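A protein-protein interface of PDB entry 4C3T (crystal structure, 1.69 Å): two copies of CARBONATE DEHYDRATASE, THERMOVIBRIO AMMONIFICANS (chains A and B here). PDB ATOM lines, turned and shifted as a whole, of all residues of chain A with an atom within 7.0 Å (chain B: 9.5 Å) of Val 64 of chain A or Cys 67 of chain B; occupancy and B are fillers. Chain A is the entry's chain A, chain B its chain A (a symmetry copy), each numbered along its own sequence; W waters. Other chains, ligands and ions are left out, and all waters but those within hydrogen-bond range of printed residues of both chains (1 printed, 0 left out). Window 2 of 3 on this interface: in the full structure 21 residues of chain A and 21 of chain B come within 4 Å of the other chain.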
ATOM      1  N   ASN A  59     -16.138   2.199 -32.581  1.00  0.00           N
ATOM      2  CA  ASN A  59     -15.869   2.895 -33.848  1.00  0.00           C
ATOM      3  C   ASN A  59     -14.922   4.090 -33.713  1.00  0.00           C
ATOM      4  O   ASN A  59     -14.504   4.435 -32.604  1.00  0.00           O
ATOM      5  CB  ASN A  59     -17.193   3.327 -34.482  1.00  0.00           C
ATOM      6  CG  ASN A  59     -18.034   4.168 -33.546  1.00  0.00           C
ATOM      7  OD1 ASN A  59     -17.587   5.197 -33.043  1.00  0.00           O
ATOM      8  ND2 ASN A  59     -19.257   3.720 -33.290  1.00  0.00           N
ATOM      9  N   SER A  60     -14.593   4.720 -34.845  1.00  0.00           N
ATOM     10  CA  SER A  60     -13.653   5.855 -34.881  1.00  0.00           C
ATOM     11  C   SER A  60     -14.132   7.083 -34.097  1.00  0.00           C
ATOM     12  O   SER A  60     -13.324   7.799 -33.487  1.00  0.00           O
ATOM     13  CB  SER A  60     -13.362   6.263 -36.328  1.00  0.00           C
ATOM     14  OG  SER A  60     -14.530   6.793 -36.936  1.00  0.00           O
ATOM     15  N   ALA A  61     -15.441   7.325 -34.115  1.00  0.00           N
ATOM     16  CA  ALA A  61     -16.009   8.495 -33.451  1.00  0.00           C
ATOM     17  C   ALA A  61     -16.069   8.332 -31.928  1.00  0.00           C
ATOM     18  O   ALA A  61     -16.055   9.325 -31.202  1.00  0.00           O
ATOM     19  CB  ALA A  61     -17.379   8.825 -34.020  1.00  0.00           C
ATOM     20  N   ASP A  62     -16.129   7.089 -31.451  1.00  0.00           N
ATOM     21  CA  ASP A  62     -16.268   6.852 -30.014  1.00  0.00           C
ATOM     22  C   ASP A  62     -15.008   6.400 -29.285  1.00  0.00           C
ATOM     23  O   ASP A  62     -15.021   6.296 -28.070  1.00  0.00           O
ATOM     24  CB  ASP A  62     -17.462   5.933 -29.693  1.00  0.00           C
ATOM     25  CG  ASP A  62     -17.234   4.453 -30.045  1.00  0.00           C
ATOM     26  OD1 ASP A  62     -16.090   3.960 -30.170  1.00  0.00           O
ATOM     27  OD2 ASP A  62     -18.262   3.760 -30.161  1.00  0.00           O
ATOM     28  N   ALA A  63     -13.933   6.150 -30.031  1.00  0.00           N
ATOM     29  CA  ALA A  63     -12.675   5.683 -29.441  1.00  0.00           C
ATOM     30  C   ALA A  63     -11.601   6.769 -29.382  1.00  0.00           C
ATOM     31  O   ALA A  63     -11.541   7.659 -30.248  1.00  0.00           O
ATOM     32  CB  ALA A  63     -12.164   4.459 -30.184  1.00  0.00           C
ATOM     33  N   VAL A  64     -10.732   6.674 -28.370  1.00  0.00           N
ATOM     34  CA  VAL A  64      -9.658   7.638 -28.150  1.00  0.00           C
ATOM     35  C   VAL A  64      -8.368   6.928 -27.729  1.00  0.00           C
ATOM     36  O   VAL A  64      -8.366   6.045 -26.874  1.00  0.00           O
ATOM     37  CB  VAL A  64     -10.083   8.759 -27.157  1.00  0.00           C
ATOM     38  CG1 VAL A  64     -10.467   8.193 -25.801  1.00  0.00           C
ATOM     39  CG2 VAL A  64      -9.006   9.828 -27.023  1.00  0.00           C
ATOM     40  N   LYS A  65      -7.276   7.302 -28.392  1.00  0.00           N
ATOM     41  CA  LYS A  65      -5.963   6.761 -28.104  1.00  0.00           C
ATOM     42  C   LYS A  65      -5.624   7.090 -26.641  1.00  0.00           C
ATOM     43  O   LYS A  65      -5.760   8.232 -26.214  1.00  0.00           O
ATOM     44  CB  LYS A  65      -4.958   7.400 -29.057  1.00  0.00           C
ATOM     45  CG  LYS A  65      -3.531   6.913 -28.938  1.00  0.00           C
ATOM     46  CD  LYS A  65      -2.670   7.530 -30.040  1.00  0.00           C
ATOM     47  CE  LYS A  65      -2.918   6.874 -31.392  1.00  0.00           C
ATOM     48  NZ  LYS A  65      -2.010   7.407 -32.457  1.00  0.00           N
ATOM     49  N   ALA A  66      -5.251   6.069 -25.885  1.00  0.00           N
ATOM     50  CA  ALA A  66      -4.965   6.225 -24.455  1.00  0.00           C
ATOM     51  C   ALA A  66      -3.800   5.338 -24.017  1.00  0.00           C
ATOM     52  O   ALA A  66      -3.546   4.294 -24.609  1.00  0.00           O
ATOM     53  CB  ALA A  66      -6.194   5.888 -23.644  1.00  0.00           C
ATOM     54  N   CYS A  67      -3.101   5.767 -22.976  1.00  0.00           N
ATOM     55  CA  CYS A  67      -1.929   5.033 -22.490  1.00  0.00           C
ATOM     56  C   CYS A  67      -2.294   3.899 -21.542  1.00  0.00           C
ATOM     57  O   CYS A  67      -1.905   3.878 -20.373  1.00  0.00           O
ATOM     58  CB  CYS A  67      -0.935   5.993 -21.840  1.00  0.00           C
ATOM     59  SG  CYS A  67      -0.423   7.320 -22.942  1.00  0.00           S
ATOM     60  N   LEU A  68      -3.025   2.927 -22.078  1.00  0.00           N
ATOM     61  CA  LEU A  68      -3.546   1.801 -21.321  1.00  0.00           C
ATOM     62  C   LEU A  68      -2.452   0.834 -20.878  1.00  0.00           C
ATOM     63  O   LEU A  68      -1.593   0.442 -21.665  1.00  0.00           O
ATOM     64  CB  LEU A  68      -4.554   1.040 -22.187  1.00  0.00           C
ATOM     65  CG  LEU A  68      -5.819   1.810 -22.581  1.00  0.00           C
ATOM     66  CD1 LEU A  68      -6.530   1.079 -23.713  1.00  0.00           C
ATOM     67  CD2 LEU A  68      -6.747   2.008 -21.393  1.00  0.00           C
ATOM     68  N   LYS A 244     -16.336   7.268 -23.528  1.00  0.00           N
ATOM     69  CA  LYS A 244     -15.351   7.046 -24.583  1.00  0.00           C
ATOM     70  C   LYS A 244     -14.839   5.620 -24.466  1.00  0.00           C
ATOM     71  O   LYS A 244     -14.704   5.078 -23.345  1.00  0.00           O
ATOM     72  CB  LYS A 244     -14.156   8.004 -24.446  1.00  0.00           C
ATOM     73  CG  LYS A 244     -14.297   9.345 -25.152  1.00  0.00           C
ATOM     74  CD  LYS A 244     -14.431   9.163 -26.659  1.00  0.00           C
ATOM     75  CE  LYS A 244     -14.284  10.466 -27.414  1.00  0.00           C
ATOM     76  NZ  LYS A 244     -14.510  10.243 -28.868  1.00  0.00           N
ATOM     77  N   VAL A 245     -14.563   4.989 -25.604  1.00  0.00           N
ATOM     78  CA  VAL A 245     -13.820   3.752 -25.604  1.00  0.00           C
ATOM     79  C   VAL A 245     -12.331   4.108 -25.732  1.00  0.00           C
ATOM     80  O   VAL A 245     -11.930   4.881 -26.600  1.00  0.00           O
ATOM     81  CB  VAL A 245     -14.235   2.825 -26.779  1.00  0.00           C
ATOM     82  CG1 VAL A 245     -13.418   1.546 -26.767  1.00  0.00           C
ATOM     83  CG2 VAL A 245     -15.731   2.546 -26.723  1.00  0.00           C
ATOM     84  N   MET A 246     -11.509   3.572 -24.840  1.00  0.00           N
ATOM     85  CA  MET A 246     -10.064   3.801 -24.908  1.00  0.00           C
ATOM     86  C   MET A 246      -9.396   2.759 -25.785  1.00  0.00           C
ATOM     87  O   MET A 246      -9.752   1.582 -25.736  1.00  0.00           O
ATOM     88  CB  MET A 246      -9.443   3.801 -23.520  1.00  0.00           C
ATOM     89  CG  MET A 246      -9.774   5.068 -22.764  1.00  0.00           C
ATOM     90  SD  MET A 246      -9.254   4.930 -21.041  1.00  0.00           S
ATOM     91  CE  MET A 246     -10.472   3.791 -20.400  1.00  0.00           C
ATOM     92  N   LYS A 247      -8.453   3.195 -26.608  1.00  0.00           N
ATOM     93  CA  LYS A 247      -7.759   2.293 -27.542  1.00  0.00           C
ATOM     94  C   LYS A 247      -6.245   2.509 -27.561  1.00  0.00           C
ATOM     95  O   LYS A 247      -5.716   3.432 -26.930  1.00  0.00           O
ATOM     96  CB  LYS A 247      -8.303   2.478 -28.964  1.00  0.00           C
ATOM     97  CG  LYS A 247      -7.912   3.794 -29.612  1.00  0.00           C
ATOM     98  CD  LYS A 247      -8.284   3.803 -31.089  1.00  0.00           C
ATOM     99  CE  LYS A 247      -7.775   5.073 -31.744  1.00  0.00           C
ATOM    100  NZ  LYS A 247      -8.199   5.148 -33.171  1.00  0.00           N
ATOM    101  OXT LYS A 247      -5.525   1.777 -28.250  1.00  0.00           O
ATOM    102  N   VAL B  64      -5.540   8.403 -16.827  1.00  0.00           N
ATOM    103  CA  VAL B  64      -4.766   7.865 -17.942  1.00  0.00           C
ATOM    104  C   VAL B  64      -4.624   8.906 -19.057  1.00  0.00           C
ATOM    105  O   VAL B  64      -5.583   9.568 -19.448  1.00  0.00           O
ATOM    106  CB  VAL B  64      -5.347   6.512 -18.447  1.00  0.00           C
ATOM    107  CG1 VAL B  64      -6.782   6.659 -18.923  1.00  0.00           C
ATOM    108  CG2 VAL B  64      -4.469   5.895 -19.528  1.00  0.00           C
ATOM    109  N   LYS B  65      -3.388   9.069 -19.521  1.00  0.00           N
ATOM    110  CA  LYS B  65      -3.071   9.986 -20.598  1.00  0.00           C
ATOM    111  C   LYS B  65      -3.867   9.552 -21.841  1.00  0.00           C
ATOM    112  O   LYS B  65      -3.854   8.381 -22.208  1.00  0.00           O
ATOM    113  CB  LYS B  65      -1.570   9.926 -20.859  1.00  0.00           C
ATOM    114  CG  LYS B  65      -1.045  10.863 -21.924  1.00  0.00           C
ATOM    115  CD  LYS B  65       0.481  10.796 -21.978  1.00  0.00           C
ATOM    116  CE  LYS B  65       1.126  11.544 -20.818  1.00  0.00           C
ATOM    117  NZ  LYS B  65       2.620  11.565 -20.916  1.00  0.00           N
ATOM    118  N   ALA B  66      -4.595  10.491 -22.424  1.00  0.00           N
ATOM    119  CA  ALA B  66      -5.457  10.202 -23.575  1.00  0.00           C
ATOM    120  C   ALA B  66      -5.459  11.357 -24.576  1.00  0.00           C
ATOM    121  O   ALA B  66      -5.248  12.508 -24.210  1.00  0.00           O
ATOM    122  CB  ALA B  66      -6.867   9.930 -23.108  1.00  0.00           C
ATOM    123  N   CYS B  67      -5.702  11.033 -25.838  1.00  0.00           N
ATOM    124  CA  CYS B  67      -5.683  12.042 -26.901  1.00  0.00           C
ATOM    125  C   CYS B  67      -7.004  12.787 -27.032  1.00  0.00           C
ATOM    126  O   CYS B  67      -7.675  12.743 -28.065  1.00  0.00           O
ATOM    127  CB  CYS B  67      -5.278  11.405 -28.229  1.00  0.00           C
ATOM    128  SG  CYS B  67      -3.690  10.562 -28.144  1.00  0.00           S
ATOM    129  N   LEU B  68      -7.353  13.510 -25.973  1.00  0.00           N
ATOM    130  CA  LEU B  68      -8.614  14.225 -25.868  1.00  0.00           C
ATOM    131  C   LEU B  68      -8.689  15.427 -26.804  1.00  0.00           C
ATOM    132  O   LEU B  68      -7.762  16.232 -26.882  1.00  0.00           O
ATOM    133  CB  LEU B  68      -8.793  14.713 -24.427  1.00  0.00           C
ATOM    134  CG  LEU B  68      -8.921  13.621 -23.359  1.00  0.00           C
ATOM    135  CD1 LEU B  68      -8.724  14.233 -21.976  1.00  0.00           C
ATOM    136  CD2 LEU B  68     -10.256  12.901 -23.450  1.00  0.00           C
ATOM    137  N   ALA B  69      -9.809  15.528 -27.512  1.00  0.00           N
ATOM    138  CA  ALA B  69     -10.072  16.630 -28.439  1.00  0.00           C
ATOM    139  C   ALA B  69     -10.172  17.972 -27.714  1.00  0.00           C
ATOM    140  O   ALA B  69     -10.702  18.035 -26.608  1.00  0.00           O
ATOM    141  CB  ALA B  69     -11.373  16.351 -29.181  1.00  0.00           C
ATOM    142  N   PRO B  70      -9.699  19.062 -28.341  1.00  0.00           N
ATOM    143  CA  PRO B  70      -9.957  20.379 -27.773  1.00  0.00           C
ATOM    144  C   PRO B  70     -11.459  20.594 -27.638  1.00  0.00           C
ATOM    145  O   PRO B  70     -12.215  20.233 -28.546  1.00  0.00           O
ATOM    146  CB  PRO B  70      -9.373  21.344 -28.821  1.00  0.00           C
ATOM    147  CG  PRO B  70      -8.376  20.530 -29.587  1.00  0.00           C
ATOM    148  CD  PRO B  70      -8.930  19.135 -29.605  1.00  0.00           C
ATOM    149  N   ASP B 102     -17.527  15.977 -28.668  1.00  0.00           N
ATOM    150  CA  ASP B 102     -17.865  14.769 -29.440  1.00  0.00           C
ATOM    151  C   ASP B 102     -18.538  15.176 -30.751  1.00  0.00           C
ATOM    152  O   ASP B 102     -19.489  14.523 -31.214  1.00  0.00           O
ATOM    153  CB  ASP B 102     -18.727  13.784 -28.636  1.00  0.00           C
ATOM    154  CG  ASP B 102     -17.980  13.211 -27.432  1.00  0.00           C
ATOM    155  OD1 ASP B 102     -16.753  13.397 -27.381  1.00  0.00           O
ATOM    156  OD2 ASP B 102     -18.611  12.563 -26.573  1.00  0.00           O
ATOM    157  N   TYR B 190      -7.910  19.485 -19.923  1.00  0.00           N
ATOM    158  CA  TYR B 190      -8.974  18.999 -19.038  1.00  0.00           C
ATOM    159  C   TYR B 190      -8.888  17.511 -18.744  1.00  0.00           C
ATOM    160  O   TYR B 190      -8.256  16.744 -19.472  1.00  0.00           O
ATOM    161  CB  TYR B 190     -10.360  19.359 -19.620  1.00  0.00           C
ATOM    162  CG  TYR B 190     -10.658  18.685 -20.941  1.00  0.00           C
ATOM    163  CD1 TYR B 190     -10.294  19.293 -22.146  1.00  0.00           C
ATOM    164  CD2 TYR B 190     -11.308  17.443 -20.980  1.00  0.00           C
ATOM    165  CE1 TYR B 190     -10.550  18.676 -23.370  1.00  0.00           C
ATOM    166  CE2 TYR B 190     -11.575  16.827 -22.191  1.00  0.00           C
ATOM    167  CZ  TYR B 190     -11.204  17.455 -23.378  1.00  0.00           C
ATOM    168  OH  TYR B 190     -11.463  16.815 -24.589  1.00  0.00           O
ATOM    169  N   ARG B 192     -11.450  14.256 -18.356  1.00  0.00           N
ATOM    170  CA  ARG B 192     -12.787  13.831 -18.781  1.00  0.00           C
ATOM    171  C   ARG B 192     -13.156  12.468 -18.223  1.00  0.00           C
ATOM    172  O   ARG B 192     -12.306  11.552 -18.155  1.00  0.00           O
ATOM    173  CB  ARG B 192     -12.895  13.821 -20.320  1.00  0.00           C
ATOM    174  CG  ARG B 192     -14.115  13.059 -20.785  1.00  0.00           C
ATOM    175  CD  ARG B 192     -14.404  13.305 -22.258  1.00  0.00           C
ATOM    176  NE  ARG B 192     -15.617  12.567 -22.593  1.00  0.00           N
ATOM    177  CZ  ARG B 192     -16.223  12.669 -23.771  1.00  0.00           C
ATOM    178  NH1 ARG B 192     -15.709  13.468 -24.690  1.00  0.00           N
ATOM    179  NH2 ARG B 192     -17.326  11.973 -24.029  1.00  0.00           N
ATOM    180  N   LYS B 244     -12.069   5.010 -15.792  1.00  0.00           N
ATOM    181  CA  LYS B 244     -10.810   5.750 -15.825  1.00  0.00           C
ATOM    182  C   LYS B 244     -11.125   7.221 -16.037  1.00  0.00           C
ATOM    183  O   LYS B 244     -12.089   7.573 -16.756  1.00  0.00           O
ATOM    184  CB  LYS B 244      -9.909   5.276 -16.977  1.00  0.00           C
ATOM    185  CG  LYS B 244      -8.976   4.117 -16.655  1.00  0.00           C
ATOM    186  CD  LYS B 244      -7.981   4.497 -15.564  1.00  0.00           C
ATOM    187  CE  LYS B 244      -6.865   3.486 -15.421  1.00  0.00           C
ATOM    188  NZ  LYS B 244      -5.977   3.862 -14.288  1.00  0.00           N
ATOM    189  N   VAL B 245     -10.343   8.096 -15.411  1.00  0.00           N
ATOM    190  CA  VAL B 245     -10.375   9.497 -15.755  1.00  0.00           C
ATOM    191  C   VAL B 245      -9.328   9.726 -16.856  1.00  0.00           C
ATOM    192  O   VAL B 245      -8.177   9.311 -16.740  1.00  0.00           O
ATOM    193  CB  VAL B 245     -10.053  10.403 -14.535  1.00  0.00           C
ATOM    194  CG1 VAL B 245     -10.069  11.867 -14.936  1.00  0.00           C
ATOM    195  CG2 VAL B 245     -11.023  10.113 -13.397  1.00  0.00           C
ATOM    196  N   MET B 246      -9.737  10.358 -17.948  1.00  0.00           N
ATOM    197  CA  MET B 246      -8.804  10.677 -19.031  1.00  0.00           C
ATOM    198  C   MET B 246      -8.149  12.024 -18.795  1.00  0.00           C
ATOM    199  O   MET B 246      -8.804  12.968 -18.355  1.00  0.00           O
ATOM    200  CB  MET B 246      -9.506  10.659 -20.381  1.00  0.00           C
ATOM    201  CG  MET B 246      -9.802   9.247 -20.833  1.00  0.00           C
ATOM    202  SD  MET B 246     -10.861   9.261 -22.296  1.00  0.00           S
ATOM    203  CE  MET B 246     -12.424   9.758 -21.588  1.00  0.00           C
ATOM    204  N   LYS B 247      -6.852  12.105 -19.057  1.00  0.00           N
ATOM    205  CA  LYS B 247      -6.089  13.344 -18.829  1.00  0.00           C
ATOM    206  C   LYS B 247      -5.160  13.691 -19.994  1.00  0.00           C
ATOM    207  O   LYS B 247      -5.011  12.924 -20.952  1.00  0.00           O
ATOM    208  CB  LYS B 247      -5.254  13.226 -17.548  1.00  0.00           C
ATOM    209  CG  LYS B 247      -4.079  12.271 -17.658  1.00  0.00           C
ATOM    210  CD  LYS B 247      -3.170  12.386 -16.441  1.00  0.00           C
ATOM    211  CE  LYS B 247      -1.941  11.517 -16.628  1.00  0.00           C
ATOM    212  NZ  LYS B 247      -1.075  11.543 -15.415  1.00  0.00           N
ATOM    213  OXT LYS B 247      -4.505  14.740 -19.970  1.00  0.00           O
HETATM  214  O   HOH W   1     -14.288  13.653 -28.981  1.00  0.00           O
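O of Lys 65 of chain A is in hydrogen-bond range of N of Cys 67 of chain B (2.8 Å).
The backbone NH of Cys 67 of chain A lies within hydrogen-bond range of the backbone carbonyl oxygen of Lys 65 of chain B (2.8 Å).
The backbone carbonyl oxygen of Val 64 of chain B sits at hydrogen-bond distance from the backbone NH of Lys 247 of chain B (2.9 Å).
O of Lys 247 of chain A lies within hydrogen-bond range of N of Ala 66 of chain A, at 2.9 Å.
The side-chain carboxylate (OD1) of Asp 102 of chain B is in salt-bridge range of the guanidinium group (NH1) of Arg 192 of chain B (2.9 Å).
The backbone NH of Ala 66 of chain B is in hydrogen-bond range of the chain-end carboxylate of Lys 247 of chain B, 2.9 Å away.
The backbone carbonyl oxygen of Val 245 of chain B sits at hydrogen-bond distance from the backbone NH of Val 64 of chain B.
O of Val 64 of chain A lies within hydrogen-bond range of N of Lys 247 of chain A (2.9 Å).
Among the printed residues, merely in contact across the chains: Val 64 of chain A with Cys 67 of chain B (3.4 Å), Val 64 of chain A with Met 246 of chain B (3.7 Å), Lys 65 of chain A with Ala 66 of chain B (3.3 Å), Ala 66 of chain A with Lys 65 of chain B (3.3 Å), Cys 67 of chain A with Val 64 of chain B (3.4 Å), Lys 244 of chain A with Asp 102 of chain B (3.8 Å), Lys 244 of chain A with Met 246 of chain B (3.8 Å), Met 246 of chain A with Val 64 of chain B (3.7 Å) and Met 246 of chain A with Lys 244 of chain B (3.8 Å).
Of the printed residues of chain B, Val 64 of chain A touches Cys 67 and Met 246.
Printed residues of chain B within 4 Å of Lys 65 of chain A: Ala 66 (3.3 Å) and Cys 67 (2.8 Å).
Printed residues of chain B within 4 Å of Cys 67 of chain A: Val 64 and Lys 65.
Of the printed residues of chain A, Lys 65 of chain B touches Ala 66 (3.3 Å) and Cys 67 (2.8 Å).
Of the printed residues of chain A, Cys 67 of chain B touches Val 64 (3.4 Å) and Lys 65 (2.8 Å).
Printed residues of chain A within 4 Å of Lys 244 of chain B: Met 246 (3.8 Å).
The nearest printed residue of chain B that does not touch Val 64 of chain A is Leu 68 of chain B (4.2 Å).
Of the 14 printed residues of chain B, 7 touch a printed residue of chain A.
Printed residues of chain B that touch a printed residue of chain A: Val 64, Lys 65, Ala 66, Cys 67, Asp 102, Lys 244 and Met 246.
Hydrophobic or aromatic side chains of chain B that line the printed part of chain A: Val 64, Ala 66 and Met 246.
Along chain B the printed residues that touch a printed residue of chain A span positions 64 to 246.
Of the 14 printed residues of chain A, 6 touch a printed residue of chain B.
Val 64 of chain A touches Cys 67 of chain B, and with the chains exchanged Cys 67 of chain A touches Val 64 of chain B.
Lys 65 of chain A touches Ala 66 of chain B, and with the chains exchanged Ala 66 of chain A touches Lys 65 of chain B.
Lys 65 of chain A touches Cys 67 of chain B, and with the chains exchanged Cys 67 of chain A touches Lys 65 of chain B.
Lys 244 of chain A touches Met 246 of chain B, and with the chains exchanged Met 246 of chain A touches Lys 244 of chain B.
9 positions are printed for both chains.
Water W1 lies within hydrogen-bond range of the side-chain carboxylate of Asp 102 of chain B (2.9 Å) and the side-chain amino group of Lys 244 of chain A (3.4 Å).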
